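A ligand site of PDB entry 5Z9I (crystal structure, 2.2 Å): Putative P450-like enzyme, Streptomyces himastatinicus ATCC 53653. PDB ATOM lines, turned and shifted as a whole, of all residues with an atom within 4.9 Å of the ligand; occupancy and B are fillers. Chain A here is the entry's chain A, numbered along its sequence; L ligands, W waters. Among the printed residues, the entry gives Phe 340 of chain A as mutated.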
ATOM      1  N   LEU A  48     -13.327  29.859  -5.756  1.00  0.00           N
ATOM      2  CA  LEU A  48     -14.719  30.311  -5.751  1.00  0.00           C
ATOM      3  C   LEU A  48     -15.011  31.187  -4.516  1.00  0.00           C
ATOM      4  O   LEU A  48     -15.886  32.055  -4.539  1.00  0.00           O
ATOM      5  CB  LEU A  48     -15.669  29.106  -5.779  1.00  0.00           C
ATOM      6  CG  LEU A  48     -15.552  28.231  -7.033  1.00  0.00           C
ATOM      7  CD1 LEU A  48     -16.495  27.023  -6.966  1.00  0.00           C
ATOM      8  CD2 LEU A  48     -15.791  29.040  -8.301  1.00  0.00           C
ATOM      9  N   SER A  56     -15.881  37.197 -11.535  1.00  0.00           N
ATOM     10  CA  SER A  56     -16.873  36.527 -12.386  1.00  0.00           C
ATOM     11  C   SER A  56     -17.157  37.356 -13.661  1.00  0.00           C
ATOM     12  O   SER A  56     -17.983  36.976 -14.514  1.00  0.00           O
ATOM     13  CB  SER A  56     -18.174  36.265 -11.618  1.00  0.00           C
ATOM     14  OG  SER A  56     -18.033  35.187 -10.666  1.00  0.00           O
ATOM     15  N   PHE A  75     -26.273  39.509 -12.544  1.00  0.00           N
ATOM     16  CA  PHE A  75     -25.346  39.467 -11.440  1.00  0.00           C
ATOM     17  C   PHE A  75     -24.425  38.218 -11.415  1.00  0.00           C
ATOM     18  O   PHE A  75     -23.435  38.221 -10.667  1.00  0.00           O
ATOM     19  CB  PHE A  75     -26.104  39.577 -10.109  1.00  0.00           C
ATOM     20  CG  PHE A  75     -27.224  38.571  -9.947  1.00  0.00           C
ATOM     21  CD1 PHE A  75     -28.476  38.773 -10.537  1.00  0.00           C
ATOM     22  CD2 PHE A  75     -27.038  37.440  -9.171  1.00  0.00           C
ATOM     23  CE1 PHE A  75     -29.499  37.856 -10.375  1.00  0.00           C
ATOM     24  CE2 PHE A  75     -28.055  36.515  -8.999  1.00  0.00           C
ATOM     25  CZ  PHE A  75     -29.295  36.717  -9.596  1.00  0.00           C
ATOM     26  N   ALA A  76     -24.716  37.199 -12.235  1.00  0.00           N
ATOM     27  CA  ALA A  76     -23.851  36.020 -12.362  1.00  0.00           C
ATOM     28  C   ALA A  76     -22.480  36.382 -12.921  1.00  0.00           C
ATOM     29  O   ALA A  76     -21.521  35.649 -12.749  1.00  0.00           O
ATOM     30  CB  ALA A  76     -24.484  34.950 -13.278  1.00  0.00           C
ATOM     31  N   HIS A  83     -22.525  43.196  -6.934  1.00  0.00           N
ATOM     32  CA  HIS A  83     -23.163  41.865  -6.907  1.00  0.00           C
ATOM     33  C   HIS A  83     -24.087  41.739  -5.713  1.00  0.00           C
ATOM     34  O   HIS A  83     -25.196  41.218  -5.844  1.00  0.00           O
ATOM     35  CB  HIS A  83     -22.163  40.718  -6.871  1.00  0.00           C
ATOM     36  CG  HIS A  83     -22.809  39.394  -6.618  1.00  0.00           C
ATOM     37  ND1 HIS A  83     -22.928  38.843  -5.355  1.00  0.00           N
ATOM     38  CD2 HIS A  83     -23.398  38.515  -7.469  1.00  0.00           C
ATOM     39  CE1 HIS A  83     -23.560  37.683  -5.441  1.00  0.00           C
ATOM     40  NE2 HIS A  83     -23.862  37.459  -6.713  1.00  0.00           N
ATOM     41  N   ARG A  87     -28.055  40.880  -6.257  1.00  0.00           N
ATOM     42  CA  ARG A  87     -28.502  39.586  -5.759  1.00  0.00           C
ATOM     43  C   ARG A  87     -29.461  39.762  -4.589  1.00  0.00           C
ATOM     44  O   ARG A  87     -30.464  39.022  -4.461  1.00  0.00           O
ATOM     45  CB  ARG A  87     -27.311  38.711  -5.345  1.00  0.00           C
ATOM     46  CG  ARG A  87     -27.726  37.522  -4.509  1.00  0.00           C
ATOM     47  CD  ARG A  87     -27.267  36.229  -5.097  1.00  0.00           C
ATOM     48  NE  ARG A  87     -27.517  35.097  -4.228  1.00  0.00           N
ATOM     49  CZ  ARG A  87     -26.980  33.895  -4.386  1.00  0.00           C
ATOM     50  NH1 ARG A  87     -26.131  33.657  -5.379  1.00  0.00           N
ATOM     51  NH2 ARG A  87     -27.274  32.926  -3.533  1.00  0.00           N
ATOM     52  N   PHE A  94     -37.707  36.725  -4.833  1.00  0.00           N
ATOM     53  CA  PHE A  94     -37.988  35.319  -4.601  1.00  0.00           C
ATOM     54  C   PHE A  94     -38.636  35.097  -3.242  1.00  0.00           C
ATOM     55  O   PHE A  94     -37.974  34.611  -2.324  1.00  0.00           O
ATOM     56  CB  PHE A  94     -36.698  34.484  -4.651  1.00  0.00           C
ATOM     57  CG  PHE A  94     -36.437  33.827  -5.975  1.00  0.00           C
ATOM     58  CD1 PHE A  94     -35.727  34.492  -6.977  1.00  0.00           C
ATOM     59  CD2 PHE A  94     -36.857  32.523  -6.207  1.00  0.00           C
ATOM     60  CE1 PHE A  94     -35.462  33.881  -8.183  1.00  0.00           C
ATOM     61  CE2 PHE A  94     -36.608  31.908  -7.397  1.00  0.00           C
ATOM     62  CZ  PHE A  94     -35.910  32.573  -8.392  1.00  0.00           C
ATOM     63  N   ILE A 138     -40.191  27.067 -14.029  1.00  0.00           N
ATOM     64  CA  ILE A 138     -39.545  28.380 -14.014  1.00  0.00           C
ATOM     65  C   ILE A 138     -40.469  29.381 -14.713  1.00  0.00           C
ATOM     66  O   ILE A 138     -40.539  30.543 -14.314  1.00  0.00           O
ATOM     67  CB  ILE A 138     -38.148  28.357 -14.665  1.00  0.00           C
ATOM     68  CG1 ILE A 138     -37.403  29.659 -14.382  1.00  0.00           C
ATOM     69  CG2 ILE A 138     -38.243  28.122 -16.173  1.00  0.00           C
ATOM     70  CD1 ILE A 138     -36.869  29.756 -12.966  1.00  0.00           C
ATOM     71  N   ARG A 233     -31.524  35.425 -17.272  1.00  0.00           N
ATOM     72  CA  ARG A 233     -30.536  34.644 -16.544  1.00  0.00           C
ATOM     73  C   ARG A 233     -31.195  33.466 -15.760  1.00  0.00           C
ATOM     74  O   ARG A 233     -30.688  32.345 -15.757  1.00  0.00           O
ATOM     75  CB  ARG A 233     -29.720  35.561 -15.611  1.00  0.00           C
ATOM     76  CG  ARG A 233     -28.890  34.836 -14.477  1.00  0.00           C
ATOM     77  CD  ARG A 233     -27.784  33.962 -15.055  1.00  0.00           C
ATOM     78  NE  ARG A 233     -26.892  34.694 -15.954  1.00  0.00           N
ATOM     79  CZ  ARG A 233     -26.239  34.139 -16.983  1.00  0.00           C
ATOM     80  NH1 ARG A 233     -26.399  32.831 -17.259  1.00  0.00           N
ATOM     81  NH2 ARG A 233     -25.440  34.876 -17.760  1.00  0.00           N
ATOM     82  N   LEU A 234     -32.340  33.738 -15.134  1.00  0.00           N
ATOM     83  CA  LEU A 234     -33.084  32.724 -14.382  1.00  0.00           C
ATOM     84  C   LEU A 234     -33.575  31.643 -15.322  1.00  0.00           C
ATOM     85  O   LEU A 234     -33.470  30.463 -15.040  1.00  0.00           O
ATOM     86  CB  LEU A 234     -34.252  33.345 -13.648  1.00  0.00           C
ATOM     87  CG  LEU A 234     -33.856  34.324 -12.535  1.00  0.00           C
ATOM     88  CD1 LEU A 234     -35.077  35.075 -12.087  1.00  0.00           C
ATOM     89  CD2 LEU A 234     -33.216  33.578 -11.378  1.00  0.00           C
ATOM     90  N   ASN A 237     -30.519  29.620 -16.510  1.00  0.00           N
ATOM     91  CA  ASN A 237     -29.898  28.884 -15.414  1.00  0.00           C
ATOM     92  C   ASN A 237     -30.863  27.853 -14.802  1.00  0.00           C
ATOM     93  O   ASN A 237     -30.447  26.924 -14.120  1.00  0.00           O
ATOM     94  CB  ASN A 237     -29.427  29.830 -14.313  1.00  0.00           C
ATOM     95  CG  ASN A 237     -28.068  30.406 -14.579  1.00  0.00           C
ATOM     96  OD1 ASN A 237     -27.648  30.536 -15.727  1.00  0.00           O
ATOM     97  ND2 ASN A 237     -27.368  30.798 -13.519  1.00  0.00           N
ATOM     98  N   GLY A 238     -32.139  28.046 -15.038  1.00  0.00           N
ATOM     99  CA  GLY A 238     -33.135  27.267 -14.333  1.00  0.00           C
ATOM    100  C   GLY A 238     -33.229  25.851 -14.865  1.00  0.00           C
ATOM    101  O   GLY A 238     -32.755  24.890 -14.224  1.00  0.00           O
ATOM    102  N   THR A 241     -30.299  22.615 -16.493  1.00  0.00           N
ATOM    103  CA  THR A 241     -29.505  21.946 -15.463  1.00  0.00           C
ATOM    104  C   THR A 241     -30.376  21.039 -14.574  1.00  0.00           C
ATOM    105  O   THR A 241     -29.954  19.961 -14.167  1.00  0.00           O
ATOM    106  CB  THR A 241     -28.795  22.951 -14.585  1.00  0.00           C
ATOM    107  OG1 THR A 241     -29.759  23.918 -14.153  1.00  0.00           O
ATOM    108  CG2 THR A 241     -27.698  23.658 -15.370  1.00  0.00           C
ATOM    109  N   THR A 242     -31.593  21.476 -14.296  1.00  0.00           N
ATOM    110  CA  THR A 242     -32.538  20.701 -13.475  1.00  0.00           C
ATOM    111  C   THR A 242     -32.993  19.477 -14.272  1.00  0.00           C
ATOM    112  O   THR A 242     -33.097  18.389 -13.727  1.00  0.00           O
ATOM    113  CB  THR A 242     -33.746  21.550 -13.031  1.00  0.00           C
ATOM    114  OG1 THR A 242     -33.303  22.669 -12.257  1.00  0.00           O
ATOM    115  CG2 THR A 242     -34.683  20.734 -12.169  1.00  0.00           C
ATOM    116  N   LEU A 245     -30.143  17.044 -14.076  1.00  0.00           N
ATOM    117  CA  LEU A 245     -30.139  16.414 -12.760  1.00  0.00           C
ATOM    118  C   LEU A 245     -31.152  15.250 -12.684  1.00  0.00           C
ATOM    119  O   LEU A 245     -30.813  14.148 -12.250  1.00  0.00           O
ATOM    120  CB  LEU A 245     -30.440  17.444 -11.663  1.00  0.00           C
ATOM    121  CG  LEU A 245     -30.541  16.861 -10.244  1.00  0.00           C
ATOM    122  CD1 LEU A 245     -29.295  16.047  -9.861  1.00  0.00           C
ATOM    123  CD2 LEU A 245     -30.731  17.983  -9.235  1.00  0.00           C
ATOM    124  N   MET A 278     -25.542  15.004  -8.375  1.00  0.00           N
ATOM    125  CA  MET A 278     -24.879  16.314  -8.557  1.00  0.00           C
ATOM    126  C   MET A 278     -23.365  16.168  -8.586  1.00  0.00           C
ATOM    127  O   MET A 278     -22.695  16.752  -9.420  1.00  0.00           O
ATOM    128  CB  MET A 278     -25.256  17.283  -7.438  1.00  0.00           C
ATOM    129  CG  MET A 278     -26.654  17.860  -7.525  1.00  0.00           C
ATOM    130  SD  MET A 278     -26.882  18.842  -9.009  1.00  0.00           S
ATOM    131  CE  MET A 278     -25.531  20.019  -8.854  1.00  0.00           C
ATOM    132  N   PRO A 283     -24.260  18.686 -13.681  1.00  0.00           N
ATOM    133  CA  PRO A 283     -24.953  19.385 -14.776  1.00  0.00           C
ATOM    134  C   PRO A 283     -24.228  20.664 -15.175  1.00  0.00           C
ATOM    135  O   PRO A 283     -24.160  20.960 -16.362  1.00  0.00           O
ATOM    136  CB  PRO A 283     -26.344  19.664 -14.194  1.00  0.00           C
ATOM    137  CG  PRO A 283     -26.543  18.519 -13.181  1.00  0.00           C
ATOM    138  CD  PRO A 283     -25.165  18.361 -12.557  1.00  0.00           C
ATOM    139  N   ILE A 284     -23.706  21.410 -14.216  1.00  0.00           N
ATOM    140  CA  ILE A 284     -22.701  22.416 -14.506  1.00  0.00           C
ATOM    141  C   ILE A 284     -21.373  21.904 -13.961  1.00  0.00           C
ATOM    142  O   ILE A 284     -21.191  21.824 -12.747  1.00  0.00           O
ATOM    143  CB  ILE A 284     -23.013  23.776 -13.873  1.00  0.00           C
ATOM    144  CG1 ILE A 284     -24.310  24.346 -14.447  1.00  0.00           C
ATOM    145  CG2 ILE A 284     -21.861  24.745 -14.149  1.00  0.00           C
ATOM    146  CD1 ILE A 284     -24.256  24.584 -15.941  1.00  0.00           C
ATOM    147  N   VAL A 287     -17.030  26.363 -14.299  1.00  0.00           N
ATOM    148  CA  VAL A 287     -17.409  27.785 -14.301  1.00  0.00           C
ATOM    149  C   VAL A 287     -16.202  28.679 -14.570  1.00  0.00           C
ATOM    150  O   VAL A 287     -15.072  28.360 -14.193  1.00  0.00           O
ATOM    151  CB  VAL A 287     -18.081  28.226 -12.970  1.00  0.00           C
ATOM    152  CG1 VAL A 287     -19.301  27.318 -12.654  1.00  0.00           C
ATOM    153  CG2 VAL A 287     -17.089  28.268 -11.823  1.00  0.00           C
ATOM    154  N   ARG A 289     -13.781  32.005 -14.523  1.00  0.00           N
ATOM    155  CA  ARG A 289     -13.311  33.118 -13.718  1.00  0.00           C
ATOM    156  C   ARG A 289     -12.235  33.879 -14.496  1.00  0.00           C
ATOM    157  O   ARG A 289     -11.609  33.325 -15.415  1.00  0.00           O
ATOM    158  CB  ARG A 289     -12.756  32.633 -12.377  1.00  0.00           C
ATOM    159  CG  ARG A 289     -13.815  32.068 -11.410  1.00  0.00           C
ATOM    160  CD  ARG A 289     -14.916  33.093 -11.144  1.00  0.00           C
ATOM    161  NE  ARG A 289     -15.784  32.691 -10.056  1.00  0.00           N
ATOM    162  CZ  ARG A 289     -16.974  32.109 -10.203  1.00  0.00           C
ATOM    163  NH1 ARG A 289     -17.446  31.848 -11.418  1.00  0.00           N
ATOM    164  NH2 ARG A 289     -17.696  31.798  -9.144  1.00  0.00           N
ATOM    165  N   LEU A 338     -19.265  20.571  -5.298  1.00  0.00           N
ATOM    166  CA  LEU A 338     -19.278  21.940  -5.828  1.00  0.00           C
ATOM    167  C   LEU A 338     -20.301  22.078  -6.967  1.00  0.00           C
ATOM    168  O   LEU A 338     -20.209  23.001  -7.789  1.00  0.00           O
ATOM    169  CB  LEU A 338     -17.864  22.329  -6.298  1.00  0.00           C
ATOM    170  CG  LEU A 338     -16.779  22.380  -5.217  1.00  0.00           C
ATOM    171  CD1 LEU A 338     -15.378  22.689  -5.768  1.00  0.00           C
ATOM    172  CD2 LEU A 338     -17.169  23.420  -4.161  1.00  0.00           C
ATOM    173  N   GLY A 339     -21.267  21.170  -7.004  1.00  0.00           N
ATOM    174  CA  GLY A 339     -22.314  21.150  -8.019  1.00  0.00           C
ATOM    175  C   GLY A 339     -23.125  22.417  -8.136  1.00  0.00           C
ATOM    176  O   GLY A 339     -23.599  22.769  -9.240  1.00  0.00           O
ATOM    177  N   PHE A 340     -23.273  23.132  -7.022  1.00  0.00           N
ATOM    178  CA  PHE A 340     -23.965  24.424  -7.032  1.00  0.00           C
ATOM    179  C   PHE A 340     -22.994  25.579  -6.784  1.00  0.00           C
ATOM    180  O   PHE A 340     -23.402  26.703  -6.463  1.00  0.00           O
ATOM    181  CB  PHE A 340     -25.070  24.444  -5.963  1.00  0.00           C
ATOM    182  CG  PHE A 340     -26.183  23.486  -6.225  1.00  0.00           C
ATOM    183  CD1 PHE A 340     -26.989  23.643  -7.342  1.00  0.00           C
ATOM    184  CD2 PHE A 340     -26.429  22.431  -5.362  1.00  0.00           C
ATOM    185  CE1 PHE A 340     -28.032  22.790  -7.594  1.00  0.00           C
ATOM    186  CE2 PHE A 340     -27.473  21.557  -5.601  1.00  0.00           C
ATOM    187  CZ  PHE A 340     -28.275  21.739  -6.740  1.00  0.00           C
ATOM    188  N   GLY A 341     -21.704  25.322  -6.919  1.00  0.00           N
ATOM    189  CA  GLY A 341     -20.734  26.389  -6.705  1.00  0.00           C
ATOM    190  C   GLY A 341     -20.458  26.575  -5.224  1.00  0.00           C
ATOM    191  O   GLY A 341     -20.766  25.677  -4.436  1.00  0.00           O
ATOM    192  N   ILE A 344     -20.219  33.579  -2.730  1.00  0.00           N
ATOM    193  CA  ILE A 344     -21.236  34.604  -2.953  1.00  0.00           C
ATOM    194  C   ILE A 344     -22.118  34.360  -4.197  1.00  0.00           C
ATOM    195  O   ILE A 344     -23.228  34.854  -4.240  1.00  0.00           O
ATOM    196  CB  ILE A 344     -20.583  36.007  -3.080  1.00  0.00           C
ATOM    197  CG1 ILE A 344     -19.745  36.115  -4.352  1.00  0.00           C
ATOM    198  CG2 ILE A 344     -19.749  36.320  -1.820  1.00  0.00           C
ATOM    199  CD1 ILE A 344     -19.257  37.539  -4.650  1.00  0.00           C
ATOM    200  N   HIS A 345     -21.636  33.596  -5.172  1.00  0.00           N
ATOM    201  CA  HIS A 345     -22.439  33.236  -6.338  1.00  0.00           C
ATOM    202  C   HIS A 345     -23.101  31.849  -6.172  1.00  0.00           C
ATOM    203  O   HIS A 345     -23.644  31.316  -7.160  1.00  0.00           O
ATOM    204  CB  HIS A 345     -21.582  33.234  -7.624  1.00  0.00           C
ATOM    205  CG  HIS A 345     -21.015  34.573  -7.970  1.00  0.00           C
ATOM    206  ND1 HIS A 345     -21.738  35.528  -8.674  1.00  0.00           N
ATOM    207  CD2 HIS A 345     -19.816  35.139  -7.709  1.00  0.00           C
ATOM    208  CE1 HIS A 345     -20.995  36.605  -8.849  1.00  0.00           C
ATOM    209  NE2 HIS A 345     -19.821  36.399  -8.267  1.00  0.00           N
ATOM    210  N   PHE A 346     -23.026  31.291  -4.968  1.00  0.00           N
ATOM    211  CA  PHE A 346     -23.683  30.025  -4.607  1.00  0.00           C
ATOM    212  C   PHE A 346     -25.071  29.971  -5.225  1.00  0.00           C
ATOM    213  O   PHE A 346     -25.876  30.874  -5.014  1.00  0.00           O
ATOM    214  CB  PHE A 346     -23.780  29.900  -3.072  1.00  0.00           C
ATOM    215  CG  PHE A 346     -23.938  28.491  -2.558  1.00  0.00           C
ATOM    216  CD1 PHE A 346     -23.583  27.399  -3.321  1.00  0.00           C
ATOM    217  CD2 PHE A 346     -24.419  28.275  -1.263  1.00  0.00           C
ATOM    218  CE1 PHE A 346     -23.710  26.096  -2.835  1.00  0.00           C
ATOM    219  CE2 PHE A 346     -24.549  26.972  -0.755  1.00  0.00           C
ATOM    220  CZ  PHE A 346     -24.208  25.885  -1.557  1.00  0.00           C
ATOM    221  N   CYS A 347     -25.346  28.930  -6.003  1.00  0.00           N
ATOM    222  CA  CYS A 347     -26.560  28.848  -6.829  1.00  0.00           C
ATOM    223  C   CYS A 347     -27.842  29.331  -6.125  1.00  0.00           C
ATOM    224  O   CYS A 347     -28.265  28.759  -5.120  1.00  0.00           O
ATOM    225  CB  CYS A 347     -26.791  27.415  -7.315  1.00  0.00           C
ATOM    226  SG  CYS A 347     -28.371  27.198  -8.112  1.00  0.00           S
ATOM    227  N   LEU A 348     -28.438  30.396  -6.665  1.00  0.00           N
ATOM    228  CA  LEU A 348     -29.621  30.987  -6.069  1.00  0.00           C
ATOM    229  C   LEU A 348     -30.847  30.040  -6.131  1.00  0.00           C
ATOM    230  O   LEU A 348     -31.740  30.124  -5.316  1.00  0.00           O
ATOM    231  CB  LEU A 348     -29.920  32.337  -6.754  1.00  0.00           C
ATOM    232  CG  LEU A 348     -31.260  33.032  -6.498  1.00  0.00           C
ATOM    233  CD1 LEU A 348     -31.147  34.534  -6.650  1.00  0.00           C
ATOM    234  CD2 LEU A 348     -32.294  32.513  -7.501  1.00  0.00           C
ATOM    235  N   GLY A 349     -30.883  29.155  -7.129  1.00  0.00           N
ATOM    236  CA  GLY A 349     -32.047  28.314  -7.350  1.00  0.00           C
ATOM    237  C   GLY A 349     -31.913  26.884  -6.853  1.00  0.00           C
ATOM    238  O   GLY A 349     -32.724  26.038  -7.226  1.00  0.00           O
ATOM    239  N   ARG A 350     -30.911  26.603  -6.020  1.00  0.00           N
ATOM    240  CA  ARG A 350     -30.640  25.209  -5.654  1.00  0.00           C
ATOM    241  C   ARG A 350     -31.756  24.541  -4.844  1.00  0.00           C
ATOM    242  O   ARG A 350     -31.991  23.349  -5.007  1.00  0.00           O
ATOM    243  CB  ARG A 350     -29.316  25.096  -4.896  1.00  0.00           C
ATOM    244  CG  ARG A 350     -29.291  25.797  -3.570  1.00  0.00           C
ATOM    245  CD  ARG A 350     -27.857  25.957  -3.082  1.00  0.00           C
ATOM    246  NE  ARG A 350     -27.828  26.420  -1.698  1.00  0.00           N
ATOM    247  CZ  ARG A 350     -27.851  27.697  -1.329  1.00  0.00           C
ATOM    248  NH1 ARG A 350     -27.908  28.652  -2.252  1.00  0.00           N
ATOM    249  NH2 ARG A 350     -27.835  28.003  -0.041  1.00  0.00           N
ATOM    250  N   LEU A 352     -34.928  25.149  -5.156  1.00  0.00           N
ATOM    251  CA  LEU A 352     -35.974  24.906  -6.118  1.00  0.00           C
ATOM    252  C   LEU A 352     -35.601  23.698  -6.981  1.00  0.00           C
ATOM    253  O   LEU A 352     -36.445  22.858  -7.269  1.00  0.00           O
ATOM    254  CB  LEU A 352     -36.207  26.154  -6.971  1.00  0.00           C
ATOM    255  N   ALA A 353     -34.335  23.595  -7.379  1.00  0.00           N
ATOM    256  CA  ALA A 353     -33.880  22.430  -8.142  1.00  0.00           C
ATOM    257  C   ALA A 353     -34.039  21.143  -7.316  1.00  0.00           C
ATOM    258  O   ALA A 353     -34.455  20.120  -7.830  1.00  0.00           O
ATOM    259  CB  ALA A 353     -32.431  22.617  -8.571  1.00  0.00           C
ATOM    260  N   GLU A 356     -37.911  20.285  -6.935  1.00  0.00           N
ATOM    261  CA  GLU A 356     -38.456  19.779  -8.195  1.00  0.00           C
ATOM    262  C   GLU A 356     -37.994  18.368  -8.487  1.00  0.00           C
ATOM    263  O   GLU A 356     -38.783  17.528  -8.920  1.00  0.00           O
ATOM    264  CB  GLU A 356     -38.027  20.638  -9.395  1.00  0.00           C
ATOM    265  CG  GLU A 356     -38.650  21.998  -9.511  1.00  0.00           C
ATOM    266  CD  GLU A 356     -38.154  22.719 -10.768  1.00  0.00           C
ATOM    267  OE1 GLU A 356     -38.392  22.205 -11.879  1.00  0.00           O
ATOM    268  OE2 GLU A 356     -37.497  23.756 -10.641  1.00  0.00           O
HETATM  269  C1  LIG L   1     -25.664  29.981 -10.023  1.00  0.00           C
HETATM  270  C2  LIG L   1     -25.722  25.339 -10.843  1.00  0.00           C
HETATM  271  C3  LIG L   1     -30.511  25.428 -10.851  1.00  0.00           C
HETATM  272  C4  LIG L   1     -30.332  30.134 -10.794  1.00  0.00           C
HETATM  273  C5  LIG L   1     -25.291  28.693 -10.168  1.00  0.00           C
HETATM  274  C6  LIG L   1     -23.978  28.277 -10.127  1.00  0.00           C
HETATM  275  C7  LIG L   1     -24.003  26.981 -10.381  1.00  0.00           C
HETATM  276  C8  LIG L   1     -25.311  26.605 -10.586  1.00  0.00           C
HETATM  277  C9  LIG L   1     -22.855  26.049 -10.451  1.00  0.00           C
HETATM  278  C10 LIG L   1     -22.785  29.153  -9.841  1.00  0.00           C
HETATM  279  C11 LIG L   1     -22.013  29.644 -11.050  1.00  0.00           C
HETATM  280  C12 LIG L   1     -20.764  30.416 -10.713  1.00  0.00           C
HETATM  281  O1  LIG L   1     -20.211  31.057 -11.550  1.00  0.00           O
HETATM  282  O2  LIG L   1     -20.277  30.403  -9.620  1.00  0.00           O
HETATM  283  C13 LIG L   1     -27.070  24.972 -10.905  1.00  0.00           C
HETATM  284  C14 LIG L   1     -27.477  23.670 -11.071  1.00  0.00           C
HETATM  285  C15 LIG L   1     -28.804  23.681 -11.075  1.00  0.00           C
HETATM  286  C16 LIG L   1     -29.205  25.042 -10.892  1.00  0.00           C
HETATM  287  C17 LIG L   1     -26.580  22.496 -11.243  1.00  0.00           C
HETATM  288  C18 LIG L   1     -29.779  22.616 -11.172  1.00  0.00           C
HETATM  289  C19 LIG L   1     -29.507  21.355 -11.070  1.00  0.00           C
HETATM  290  C20 LIG L   1     -30.893  26.727 -10.835  1.00  0.00           C
HETATM  291  C21 LIG L   1     -32.173  27.192 -10.874  1.00  0.00           C
HETATM  292  C22 LIG L   1     -32.102  28.528 -10.879  1.00  0.00           C
HETATM  293  C23 LIG L   1     -30.778  28.858 -10.844  1.00  0.00           C
HETATM  294  C24 LIG L   1     -33.381  26.339 -10.917  1.00  0.00           C
HETATM  295  C25 LIG L   1     -33.152  29.534 -10.863  1.00  0.00           C
HETATM  296  C26 LIG L   1     -34.401  29.307 -10.638  1.00  0.00           C
HETATM  297  C27 LIG L   1     -29.022  30.448 -10.572  1.00  0.00           C
HETATM  298  C28 LIG L   1     -28.604  31.800 -10.471  1.00  0.00           C
HETATM  299  C29 LIG L   1     -27.325  31.759 -10.240  1.00  0.00           C
HETATM  300  C30 LIG L   1     -26.955  30.373 -10.211  1.00  0.00           C
HETATM  301  C31 LIG L   1     -29.448  33.018 -10.589  1.00  0.00           C
HETATM  302  C32 LIG L   1     -26.453  32.954 -10.092  1.00  0.00           C
HETATM  303  C33 LIG L   1     -26.145  33.313  -8.666  1.00  0.00           C
HETATM  304  C34 LIG L   1     -25.125  34.389  -8.534  1.00  0.00           C
HETATM  305  O3  LIG L   1     -24.302  34.650  -9.379  1.00  0.00           O
HETATM  306  O4  LIG L   1     -25.089  35.029  -7.542  1.00  0.00           O
HETATM  307  N1  LIG L   1     -26.086  27.666 -10.462  1.00  0.00           N
HETATM  308  N2  LIG L   1     -28.110  25.739 -10.794  1.00  0.00           N
HETATM  309  N3  LIG L   1     -30.061  27.745 -10.816  1.00  0.00           N
HETATM  310  N4  LIG L   1     -28.014  29.621 -10.418  1.00  0.00           N
HETATM  311 FE1  LIG L   1     -28.030  27.777 -10.485  1.00  0.00          FE
HETATM  312  O   HOH W   1     -27.554  27.533 -12.952  1.00  0.00           O
HETATM  313  O   HOH W   2     -24.620  28.403 -13.556  1.00  0.00           O
HETATM  314  O   HOH W   3     -20.084  33.854 -11.228  1.00  0.00           O
HETATM  315  O   HOH W   4     -20.823  32.172 -14.370  1.00  0.00           O
HETATM  316  O   HOH W   5     -20.162  29.760  -6.999  1.00  0.00           O
HETATM  317  O   HOH W   6     -22.865  32.822 -11.478  1.00  0.00           O
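The side-chain sulfur of Cys 347 binds an iron atom (FE1) of the ligand (2.5 Å). An oxygen (O4) of the ligand is in salt-bridge range of the guanidinium group (NH1) of Arg 87 (2.8 Å). O3 of the ligand sits at hydrogen-bond distance from ND1 of His 345 (2.8 Å). A ring nitrogen (NE2) of His 83 lies within hydrogen-bond range of an oxygen (O4) of the ligand, at 2.8 Å. The guanidinium group (NH1) of Arg 289 lies within salt-bridge range of an oxygen (O1) of the ligand (2.9 Å).
The backbone NH of Cys 347 is in hydrogen-bond range of the backbone carbonyl oxygen of Phe 340. The backbone carbonyl oxygen (O) of Cys 347 is in hydrogen-bond range of the guanidinium group (NH1) of Arg 350. The guanidinium group of Arg 87 sits at hydrogen-bond distance from the backbone carbonyl oxygen of Ile 344 (3.3 Å). The backbone carbonyl oxygen (O) of Phe 346 sits at hydrogen-bond distance from the guanidinium group (NH1) of Arg 87 (2.8 Å). A ring nitrogen (ND1) of His 345 sits at hydrogen-bond distance from a ring nitrogen (NE2) of His 83. A ring nitrogen (NE2) of His 345 sits at hydrogen-bond distance from the side-chain hydroxyl of Ser 56, 3.2 Å away. The side-chain hydroxyl of Thr 241 lies within hydrogen-bond range of the backbone carbonyl oxygen of Asn 237 (3.1 Å). The side-chain hydroxyl (OG1) of Thr 242 lies within hydrogen-bond range of the backbone carbonyl oxygen (O) of Gly 238.
A nitrogen (N4) of the ligand lies close to the side-chain amide nitrogen (ND2) of Asn 237 (3.4 Å). CD2 of Phe 75 touches O4 of the ligand (3.5 Å). CA of Ala 76 touches O3 of the ligand, at 3.3 Å. Ile 138 touches the ligand. Leu 234 touches the ligand (CD2 to C31, 3.9 Å). Gly 238 touches the ligand. Thr 241 touches the ligand. Thr 242 touches the ligand (OG1 to C18, 3.7 Å). CE of Met 278 touches C17 of the ligand, 3.6 Å away. CG1 of Ile 284 touches C2 of the ligand (3.996 Å). Val 287 touches the ligand. O of Gly 339 touches C9 of the ligand, 3.6 Å away. Phe 340 touches the ligand (CE1 to C14, 3.6 Å). Gly 341 touches the ligand. Ile 344 touches the ligand (O to O4, 3.8 Å). N of Leu 348 touches C30 of the ligand (3.8 Å). CA of Gly 349 touches C22 of the ligand, at 3.5 Å. Ala 353 touches the ligand (CB to C18, 3.7 Å). Hydrophobic or aromatic side chains that line the ligand: Phe 75, Ala 76, His 83, Ile 138, Leu 234, Met 278, Ile 284, Val 287, Phe 340, His 345, Leu 348 and Ala 353. 23 residues have an atom within 4 Å of the ligand: Phe 75, Ala 76, His 83, Arg 87, Ile 138, Leu 234, Asn 237, Gly 238, Thr 241, Thr 242, Met 278, Ile 284, Val 287, Arg 289, Gly 339, Phe 340, Gly 341, Ile 344, His 345, Cys 347, Leu 348, Gly 349 and Ala 353.
Water W3 lies within hydrogen-bond range of OG of Ser 56, O of Ala 76, O1 of the ligand, NH1 of Arg 289 and ND1 of His 345. Water W6 bridges an oxygen (O3) of the ligand (3.1 Å) and the backbone carbonyl oxygen (O) of Ala 76 (3.4 Å).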
